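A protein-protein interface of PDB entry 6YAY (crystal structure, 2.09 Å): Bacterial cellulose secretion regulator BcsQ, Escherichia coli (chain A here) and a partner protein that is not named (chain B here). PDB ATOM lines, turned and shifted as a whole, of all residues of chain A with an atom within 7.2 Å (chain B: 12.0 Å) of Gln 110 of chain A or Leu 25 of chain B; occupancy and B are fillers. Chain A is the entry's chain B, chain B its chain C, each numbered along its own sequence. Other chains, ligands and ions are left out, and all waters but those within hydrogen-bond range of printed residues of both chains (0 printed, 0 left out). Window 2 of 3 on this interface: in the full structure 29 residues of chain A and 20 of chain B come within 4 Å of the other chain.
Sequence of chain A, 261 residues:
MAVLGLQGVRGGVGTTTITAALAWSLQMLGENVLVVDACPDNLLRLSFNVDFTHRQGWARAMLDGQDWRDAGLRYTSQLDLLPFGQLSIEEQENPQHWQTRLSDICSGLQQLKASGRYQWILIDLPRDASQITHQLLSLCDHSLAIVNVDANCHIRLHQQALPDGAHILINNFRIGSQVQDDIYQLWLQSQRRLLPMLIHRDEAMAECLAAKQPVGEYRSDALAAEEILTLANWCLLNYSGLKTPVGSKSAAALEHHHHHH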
ATOM      1  N   VAL A   3      -2.432 -26.170  -5.949  1.00  0.00           N
ATOM      2  CA  VAL A   3      -2.465 -26.206  -4.491  1.00  0.00           C
ATOM      3  C   VAL A   3      -3.588 -25.295  -4.016  1.00  0.00           C
ATOM      4  O   VAL A   3      -3.573 -24.086  -4.277  1.00  0.00           O
ATOM      5  CB  VAL A   3      -1.119 -25.783  -3.885  1.00  0.00           C
ATOM      6  CG1 VAL A   3      -1.186 -25.862  -2.368  1.00  0.00           C
ATOM      7  CG2 VAL A   3      -0.004 -26.655  -4.420  1.00  0.00           C
ATOM      8  N   TRP A  68       9.030 -36.549   7.551  1.00  0.00           N
ATOM      9  CA  TRP A  68       7.602 -36.310   7.394  1.00  0.00           C
ATOM     10  C   TRP A  68       7.018 -37.072   6.214  1.00  0.00           C
ATOM     11  O   TRP A  68       5.819 -37.366   6.213  1.00  0.00           O
ATOM     12  CB  TRP A  68       7.334 -34.814   7.222  1.00  0.00           C
ATOM     13  CG  TRP A  68       7.866 -34.246   5.944  1.00  0.00           C
ATOM     14  CD1 TRP A  68       9.098 -33.695   5.743  1.00  0.00           C
ATOM     15  CD2 TRP A  68       7.183 -34.171   4.686  1.00  0.00           C
ATOM     16  NE1 TRP A  68       9.224 -33.281   4.439  1.00  0.00           N
ATOM     17  CE2 TRP A  68       8.063 -33.563   3.769  1.00  0.00           C
ATOM     18  CE3 TRP A  68       5.913 -34.561   4.245  1.00  0.00           C
ATOM     19  CZ2 TRP A  68       7.717 -33.336   2.439  1.00  0.00           C
ATOM     20  CZ3 TRP A  68       5.570 -34.334   2.922  1.00  0.00           C
ATOM     21  CH2 TRP A  68       6.469 -33.728   2.036  1.00  0.00           C
ATOM     22  N   ASP A 104      10.275 -26.693   7.616  1.00  0.00           N
ATOM     23  CA  ASP A 104      10.723 -27.591   6.556  1.00  0.00           C
ATOM     24  C   ASP A 104       9.570 -28.138   5.727  1.00  0.00           C
ATOM     25  O   ASP A 104       9.796 -28.577   4.593  1.00  0.00           O
ATOM     26  CB  ASP A 104      11.525 -28.753   7.144  1.00  0.00           C
ATOM     27  CG  ASP A 104      12.920 -28.340   7.584  1.00  0.00           C
ATOM     28  OD1 ASP A 104      13.320 -27.188   7.312  1.00  0.00           O
ATOM     29  OD2 ASP A 104      13.616 -29.172   8.204  1.00  0.00           O
ATOM     30  N   ILE A 105       8.344 -28.127   6.256  1.00  0.00           N
ATOM     31  CA  ILE A 105       7.215 -28.654   5.496  1.00  0.00           C
ATOM     32  C   ILE A 105       6.958 -27.808   4.256  1.00  0.00           C
ATOM     33  O   ILE A 105       6.475 -28.316   3.236  1.00  0.00           O
ATOM     34  CB  ILE A 105       5.958 -28.751   6.387  1.00  0.00           C
ATOM     35  CG1 ILE A 105       4.891 -29.627   5.725  1.00  0.00           C
ATOM     36  CG2 ILE A 105       5.386 -27.379   6.664  1.00  0.00           C
ATOM     37  CD1 ILE A 105       5.323 -31.064   5.527  1.00  0.00           C
ATOM     38  N   CYS A 106       7.280 -26.512   4.312  1.00  0.00           N
ATOM     39  CA  CYS A 106       7.084 -25.656   3.147  1.00  0.00           C
ATOM     40  C   CYS A 106       8.038 -26.036   2.027  1.00  0.00           C
ATOM     41  O   CYS A 106       7.637 -26.112   0.860  1.00  0.00           O
ATOM     42  CB  CYS A 106       7.276 -24.194   3.532  1.00  0.00           C
ATOM     43  SG  CYS A 106       6.616 -23.802   5.147  1.00  0.00           S
ATOM     44  N   SER A 107       9.307 -26.270   2.367  1.00  0.00           N
ATOM     45  CA  SER A 107      10.261 -26.759   1.382  1.00  0.00           C
ATOM     46  C   SER A 107       9.843 -28.124   0.850  1.00  0.00           C
ATOM     47  O   SER A 107       9.928 -28.381  -0.357  1.00  0.00           O
ATOM     48  CB  SER A 107      11.659 -26.824   1.999  1.00  0.00           C
ATOM     49  OG  SER A 107      12.561 -27.516   1.154  1.00  0.00           O
ATOM     50  N   GLY A 108       9.381 -29.007   1.736  1.00  0.00           N
ATOM     51  CA  GLY A 108       8.991 -30.338   1.305  1.00  0.00           C
ATOM     52  C   GLY A 108       7.777 -30.326   0.398  1.00  0.00           C
ATOM     53  O   GLY A 108       7.723 -31.059  -0.593  1.00  0.00           O
ATOM     54  N   LEU A 109       6.786 -29.494   0.722  1.00  0.00           N
ATOM     55  CA  LEU A 109       5.621 -29.365  -0.143  1.00  0.00           C
ATOM     56  C   LEU A 109       5.941 -28.614  -1.426  1.00  0.00           C
ATOM     57  O   LEU A 109       5.247 -28.804  -2.431  1.00  0.00           O
ATOM     58  CB  LEU A 109       4.485 -28.672   0.609  1.00  0.00           C
ATOM     59  CG  LEU A 109       3.832 -29.525   1.697  1.00  0.00           C
ATOM     60  CD1 LEU A 109       2.733 -28.749   2.410  1.00  0.00           C
ATOM     61  CD2 LEU A 109       3.281 -30.808   1.093  1.00  0.00           C
ATOM     62  N   GLN A 110       6.973 -27.768  -1.413  1.00  0.00           N
ATOM     63  CA  GLN A 110       7.408 -27.108  -2.640  1.00  0.00           C
ATOM     64  C   GLN A 110       7.993 -28.111  -3.627  1.00  0.00           C
ATOM     65  O   GLN A 110       7.740 -28.023  -4.835  1.00  0.00           O
ATOM     66  CB  GLN A 110       8.434 -26.023  -2.314  1.00  0.00           C
ATOM     67  CG  GLN A 110       8.601 -24.987  -3.408  1.00  0.00           C
ATOM     68  CD  GLN A 110       7.497 -23.952  -3.388  1.00  0.00           C
ATOM     69  OE1 GLN A 110       7.484 -23.065  -2.539  1.00  0.00           O
ATOM     70  NE2 GLN A 110       6.560 -24.064  -4.321  1.00  0.00           N
ATOM     71  N   GLN A 111       8.788 -29.065  -3.132  1.00  0.00           N
ATOM     72  CA  GLN A 111       9.309 -30.122  -3.994  1.00  0.00           C
ATOM     73  C   GLN A 111       8.177 -30.960  -4.567  1.00  0.00           C
ATOM     74  O   GLN A 111       8.159 -31.273  -5.762  1.00  0.00           O
ATOM     75  CB  GLN A 111      10.268 -31.017  -3.213  1.00  0.00           C
ATOM     76  CG  GLN A 111      11.412 -30.305  -2.538  1.00  0.00           C
ATOM     77  CD  GLN A 111      12.284 -31.267  -1.766  1.00  0.00           C
ATOM     78  OE1 GLN A 111      11.987 -31.609  -0.622  1.00  0.00           O
ATOM     79  NE2 GLN A 111      13.357 -31.728  -2.397  1.00  0.00           N
ATOM     80  N   LEU A 112       7.231 -31.353  -3.711  1.00  0.00           N
ATOM     81  CA  LEU A 112       6.094 -32.149  -4.158  1.00  0.00           C
ATOM     82  C   LEU A 112       5.301 -31.412  -5.228  1.00  0.00           C
ATOM     83  O   LEU A 112       4.888 -32.006  -6.230  1.00  0.00           O
ATOM     84  CB  LEU A 112       5.212 -32.482  -2.956  1.00  0.00           C
ATOM     85  CG  LEU A 112       4.371 -33.752  -2.964  1.00  0.00           C
ATOM     86  CD1 LEU A 112       5.137 -34.907  -3.572  1.00  0.00           C
ATOM     87  CD2 LEU A 112       3.962 -34.074  -1.537  1.00  0.00           C
ATOM     88  N   LYS A 113       5.101 -30.107  -5.036  1.00  0.00           N
ATOM     89  CA  LYS A 113       4.413 -29.291  -6.030  1.00  0.00           C
ATOM     90  C   LYS A 113       5.174 -29.266  -7.352  1.00  0.00           C
ATOM     91  O   LYS A 113       4.575 -29.397  -8.426  1.00  0.00           O
ATOM     92  CB  LYS A 113       4.227 -27.878  -5.475  1.00  0.00           C
ATOM     93  CG  LYS A 113       3.424 -26.924  -6.336  1.00  0.00           C
ATOM     94  CD  LYS A 113       3.281 -25.581  -5.624  1.00  0.00           C
ATOM     95  CE  LYS A 113       2.573 -24.551  -6.488  1.00  0.00           C
ATOM     96  NZ  LYS A 113       2.553 -23.215  -5.826  1.00  0.00           N
ATOM     97  N   ALA A 114       6.501 -29.113  -7.292  1.00  0.00           N
ATOM     98  CA  ALA A 114       7.294 -29.049  -8.516  1.00  0.00           C
ATOM     99  C   ALA A 114       7.317 -30.385  -9.246  1.00  0.00           C
ATOM    100  O   ALA A 114       7.441 -30.414 -10.477  1.00  0.00           O
ATOM    101  CB  ALA A 114       8.723 -28.596  -8.198  1.00  0.00           C
ATOM    102  N   SER A 115       7.207 -31.496  -8.516  1.00  0.00           N
ATOM    103  CA  SER A 115       7.268 -32.808  -9.148  1.00  0.00           C
ATOM    104  C   SER A 115       6.016 -33.120  -9.955  1.00  0.00           C
ATOM    105  O   SER A 115       6.049 -34.018 -10.803  1.00  0.00           O
ATOM    106  CB  SER A 115       7.482 -33.895  -8.095  1.00  0.00           C
ATOM    107  OG  SER A 115       6.325 -34.051  -7.290  1.00  0.00           O
ATOM    108  N   GLY A 116       4.922 -32.403  -9.717  1.00  0.00           N
ATOM    109  CA  GLY A 116       3.676 -32.721 -10.384  1.00  0.00           C
ATOM    110  C   GLY A 116       3.138 -34.087 -10.044  1.00  0.00           C
ATOM    111  O   GLY A 116       2.356 -34.647 -10.817  1.00  0.00           O
ATOM    112  N   HIS A 134       0.780 -19.086   7.826  1.00  0.00           N
ATOM    113  CA  HIS A 134       1.093 -18.152   6.750  1.00  0.00           C
ATOM    114  C   HIS A 134       2.065 -18.755   5.745  1.00  0.00           C
ATOM    115  O   HIS A 134       2.032 -18.401   4.561  1.00  0.00           O
ATOM    116  CB  HIS A 134       1.670 -16.859   7.324  1.00  0.00           C
ATOM    117  CG  HIS A 134       0.687 -16.060   8.117  1.00  0.00           C
ATOM    118  ND1 HIS A 134       1.069 -15.082   9.008  1.00  0.00           N
ATOM    119  CD2 HIS A 134      -0.667 -16.093   8.151  1.00  0.00           C
ATOM    120  CE1 HIS A 134      -0.007 -14.547   9.558  1.00  0.00           C
ATOM    121  NE2 HIS A 134      -1.072 -15.142   9.055  1.00  0.00           N
ATOM    122  N   GLN A 135       2.933 -19.663   6.196  1.00  0.00           N
ATOM    123  CA  GLN A 135       3.898 -20.271   5.287  1.00  0.00           C
ATOM    124  C   GLN A 135       3.217 -21.222   4.310  1.00  0.00           C
ATOM    125  O   GLN A 135       3.563 -21.252   3.123  1.00  0.00           O
ATOM    126  CB  GLN A 135       4.981 -20.996   6.086  1.00  0.00           C
ATOM    127  CG  GLN A 135       6.099 -20.097   6.592  1.00  0.00           C
ATOM    128  CD  GLN A 135       7.086 -20.838   7.473  1.00  0.00           C
ATOM    129  OE1 GLN A 135       6.710 -21.745   8.216  1.00  0.00           O
ATOM    130  NE2 GLN A 135       8.354 -20.459   7.390  1.00  0.00           N
ATOM    131  N   SER A 138       1.251 -19.366   1.591  1.00  0.00           N
ATOM    132  CA  SER A 138       2.083 -18.842   0.514  1.00  0.00           C
ATOM    133  C   SER A 138       2.327 -19.869  -0.585  1.00  0.00           C
ATOM    134  O   SER A 138       2.587 -19.483  -1.728  1.00  0.00           O
ATOM    135  CB  SER A 138       3.417 -18.353   1.078  1.00  0.00           C
ATOM    136  OG  SER A 138       4.098 -19.389   1.760  1.00  0.00           O
ATOM    137  N   LEU A 139       2.238 -21.165  -0.268  1.00  0.00           N
ATOM    138  CA  LEU A 139       2.369 -22.210  -1.274  1.00  0.00           C
ATOM    139  C   LEU A 139       1.104 -22.392  -2.102  1.00  0.00           C
ATOM    140  O   LEU A 139       1.167 -23.003  -3.173  1.00  0.00           O
ATOM    141  CB  LEU A 139       2.718 -23.544  -0.610  1.00  0.00           C
ATOM    142  CG  LEU A 139       3.858 -23.557   0.409  1.00  0.00           C
ATOM    143  CD1 LEU A 139       3.942 -24.908   1.101  1.00  0.00           C
ATOM    144  CD2 LEU A 139       5.175 -23.217  -0.260  1.00  0.00           C
ATOM    145  N   CYS A 140      -0.035 -21.890  -1.631  1.00  0.00           N
ATOM    146  CA  CYS A 140      -1.299 -22.141  -2.308  1.00  0.00           C
ATOM    147  C   CYS A 140      -1.424 -21.292  -3.565  1.00  0.00           C
ATOM    148  O   CYS A 140      -1.068 -20.112  -3.579  1.00  0.00           O
ATOM    149  CB  CYS A 140      -2.476 -21.850  -1.370  1.00  0.00           C
ATOM    150  SG  CYS A 140      -2.591 -22.932   0.073  1.00  0.00           S
ATOM    151  N   ILE B  17       1.358  -8.356   4.255  1.00  0.00           N
ATOM    152  CA  ILE B  17       2.348  -9.010   3.409  1.00  0.00           C
ATOM    153  C   ILE B  17       3.279  -9.873   4.254  1.00  0.00           C
ATOM    154  O   ILE B  17       4.149  -9.362   4.959  1.00  0.00           O
ATOM    155  CB  ILE B  17       3.149  -7.981   2.592  1.00  0.00           C
ATOM    156  CG1 ILE B  17       2.211  -7.161   1.704  1.00  0.00           C
ATOM    157  CG2 ILE B  17       4.212  -8.676   1.754  1.00  0.00           C
ATOM    158  CD1 ILE B  17       2.918  -6.122   0.859  1.00  0.00           C
ATOM    159  N   PHE B  18       3.083 -11.187   4.180  1.00  0.00           N
ATOM    160  CA  PHE B  18       3.919 -12.138   4.898  1.00  0.00           C
ATOM    161  C   PHE B  18       5.135 -12.500   4.057  1.00  0.00           C
ATOM    162  O   PHE B  18       5.036 -12.658   2.838  1.00  0.00           O
ATOM    163  CB  PHE B  18       3.120 -13.399   5.244  1.00  0.00           C
ATOM    164  CG  PHE B  18       3.938 -14.478   5.896  1.00  0.00           C
ATOM    165  CD1 PHE B  18       4.259 -14.406   7.243  1.00  0.00           C
ATOM    166  CD2 PHE B  18       4.378 -15.569   5.164  1.00  0.00           C
ATOM    167  CE1 PHE B  18       5.009 -15.401   7.847  1.00  0.00           C
ATOM    168  CE2 PHE B  18       5.128 -16.567   5.761  1.00  0.00           C
ATOM    169  CZ  PHE B  18       5.444 -16.482   7.105  1.00  0.00           C
ATOM    170  N   GLN B  19       6.283 -12.625   4.715  1.00  0.00           N
ATOM    171  CA  GLN B  19       7.521 -12.974   4.029  1.00  0.00           C
ATOM    172  C   GLN B  19       8.154 -14.221   4.641  1.00  0.00           C
ATOM    173  O   GLN B  19       8.175 -15.285   4.022  1.00  0.00           O
ATOM    174  CB  GLN B  19       8.509 -11.805   4.074  1.00  0.00           C
ATOM    175  CG  GLN B  19       7.971 -10.516   3.474  1.00  0.00           C
ATOM    176  CD  GLN B  19       9.004  -9.408   3.442  1.00  0.00           C
ATOM    177  OE1 GLN B  19      10.200  -9.654   3.606  1.00  0.00           O
ATOM    178  NE2 GLN B  19       8.548  -8.179   3.232  1.00  0.00           N
ATOM    179  N   LEU B  25       8.963 -16.637  -1.107  1.00  0.00           N
ATOM    180  CA  LEU B  25       7.539 -16.467  -1.370  1.00  0.00           C
ATOM    181  C   LEU B  25       6.920 -15.436  -0.429  1.00  0.00           C
ATOM    182  O   LEU B  25       7.286 -15.353   0.743  1.00  0.00           O
ATOM    183  CB  LEU B  25       6.806 -17.803  -1.234  1.00  0.00           C
ATOM    184  CG  LEU B  25       7.351 -18.989  -2.030  1.00  0.00           C
ATOM    185  CD1 LEU B  25       6.391 -20.159  -1.922  1.00  0.00           C
ATOM    186  CD2 LEU B  25       7.590 -18.616  -3.485  1.00  0.00           C
ATOM    187  N   LYS B  26       5.973 -14.658  -0.949  1.00  0.00           N
ATOM    188  CA  LYS B  26       5.301 -13.617  -0.183  1.00  0.00           C
ATOM    189  C   LYS B  26       3.795 -13.778  -0.319  1.00  0.00           C
ATOM    190  O   LYS B  26       3.273 -13.827  -1.437  1.00  0.00           O
ATOM    191  CB  LYS B  26       5.732 -12.221  -0.646  1.00  0.00           C
ATOM    192  N   GLN B  27       3.104 -13.856   0.815  1.00  0.00           N
ATOM    193  CA  GLN B  27       1.652 -13.980   0.856  1.00  0.00           C
ATOM    194  C   GLN B  27       1.066 -12.693   1.421  1.00  0.00           C
ATOM    195  O   GLN B  27       1.374 -12.312   2.555  1.00  0.00           O
ATOM    196  CB  GLN B  27       1.228 -15.181   1.704  1.00  0.00           C
ATOM    197  CG  GLN B  27      -0.278 -15.381   1.788  1.00  0.00           C
ATOM    198  CD  GLN B  27      -0.887 -15.799   0.464  1.00  0.00           C
ATOM    199  OE1 GLN B  27      -0.394 -16.713  -0.197  1.00  0.00           O
ATOM    200  NE2 GLN B  27      -1.960 -15.126   0.067  1.00  0.00           N
ATOM    201  N   ALA B  28       0.227 -12.029   0.632  1.00  0.00           N
ATOM    202  CA  ALA B  28      -0.405 -10.782   1.033  1.00  0.00           C
ATOM    203  C   ALA B  28      -1.809 -11.043   1.562  1.00  0.00           C
ATOM    204  O   ALA B  28      -2.467 -12.017   1.182  1.00  0.00           O
ATOM    205  CB  ALA B  28      -0.460  -9.797  -0.136  1.00  0.00           C
ATOM    206  N   PHE B  29      -2.264 -10.158   2.446  1.00  0.00           N
ATOM    207  CA  PHE B  29      -3.572 -10.272   3.076  1.00  0.00           C
ATOM    208  C   PHE B  29      -4.334  -8.970   2.888  1.00  0.00           C
ATOM    209  O   PHE B  29      -3.775  -7.886   3.084  1.00  0.00           O
ATOM    210  CB  PHE B  29      -3.438 -10.603   4.566  1.00  0.00           C
ATOM    211  CG  PHE B  29      -2.872 -11.968   4.834  1.00  0.00           C
ATOM    212  CD1 PHE B  29      -3.711 -13.058   4.999  1.00  0.00           C
ATOM    213  CD2 PHE B  29      -1.503 -12.163   4.919  1.00  0.00           C
ATOM    214  CE1 PHE B  29      -3.197 -14.315   5.246  1.00  0.00           C
ATOM    215  CE2 PHE B  29      -0.980 -13.420   5.163  1.00  0.00           C
ATOM    216  CZ  PHE B  29      -1.830 -14.499   5.326  1.00  0.00           C
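The side-chain sulfur (SG) of Cys 106 of chain A lies close to the side-chain amide oxygen (OE1) of Gln 135 of chain A (3.7 Å).
The side-chain amino group (NZ) of Lys 113 of chain A lies within hydrogen-bond range of the backbone carbonyl oxygen (O) of Leu 139 of chain A (3.0 Å).
The backbone NH (N) of Phe 18 of chain B is in hydrogen-bond range of the backbone carbonyl oxygen (O) of Gln 27 of chain B (2.6 Å).
Leu 25 of chain B touches Gln 110 of chain A.
His 134 of chain A touches Phe 18 of chain B (CB to CD1, 3.6 Å).
Phe 29 of chain B touches His 134 of chain A.
Gln 135 of chain A touches Phe 18 of chain B.
Leu 25 of chain B touches Ser 138 of chain A.
Gln 27 of chain B touches Ser 138 of chain A (OE1 to CA, 3.3 Å).
CD1 of Leu 25 of chain B touches CD2 of Leu 139 of chain A (3.7 Å).
Of chain B, only Leu 25 (3.2 Å) comes within 4 Å of Gln 110 of chain A.
Leu 25 of chain B touches three residues of chain A.
No residue of chain B comes within 4 Å of Cys 106 of chain A.
Gly 108 of chain A touches none of the printed residues of chain B.
No residue of chain B comes within 4 Å of Leu 109 of chain A.
No residue of chain B comes within 4 Å of Gln 111 of chain A.
Ala 114 of chain A touches none of the printed residues of chain B.
Ser 138 of chain A touches two residues of chain B.
Leu 139 of chain A touches one residue of chain B.
Of the printed residues of chain A, Phe 18 of chain B touches His 134 and Gln 135.
Of the printed residues of chain B, His 134 of chain A touches Phe 18 and Phe 29.
Val 3 of chain A touches none of the printed residues of chain B.
The nearest residue of chain B that does not touch Gln 110 of chain A is Lys 26 of chain B (8.7 Å).
The nearest residue of chain A that does not touch Leu 25 of chain B is Gln 135 of chain A (5.9 Å).
The nearest printed residue of chain A that does not touch Phe 29 of chain B is Ser 138 of chain A (6.9 Å).
Hydrophobic or aromatic side chains of chain B within 4 Å of the printed part of chain A: Phe 18, Leu 25 and Phe 29.
Of the 20 printed residues of chain A, 5 touch a printed residue of chain B.
Printed residues of chain A that touch a printed residue of chain B: Gln 110, His 134, Gln 135, Ser 138 and Leu 139.
Hydrophobic or aromatic side chains of chain A within 4 Å of the printed part of chain B: His 134 and Leu 139.
Along chain A the printed residues that touch a printed residue of chain B span positions 110 to 139.
Among the printed residues, 7 pairs touch across the chains.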
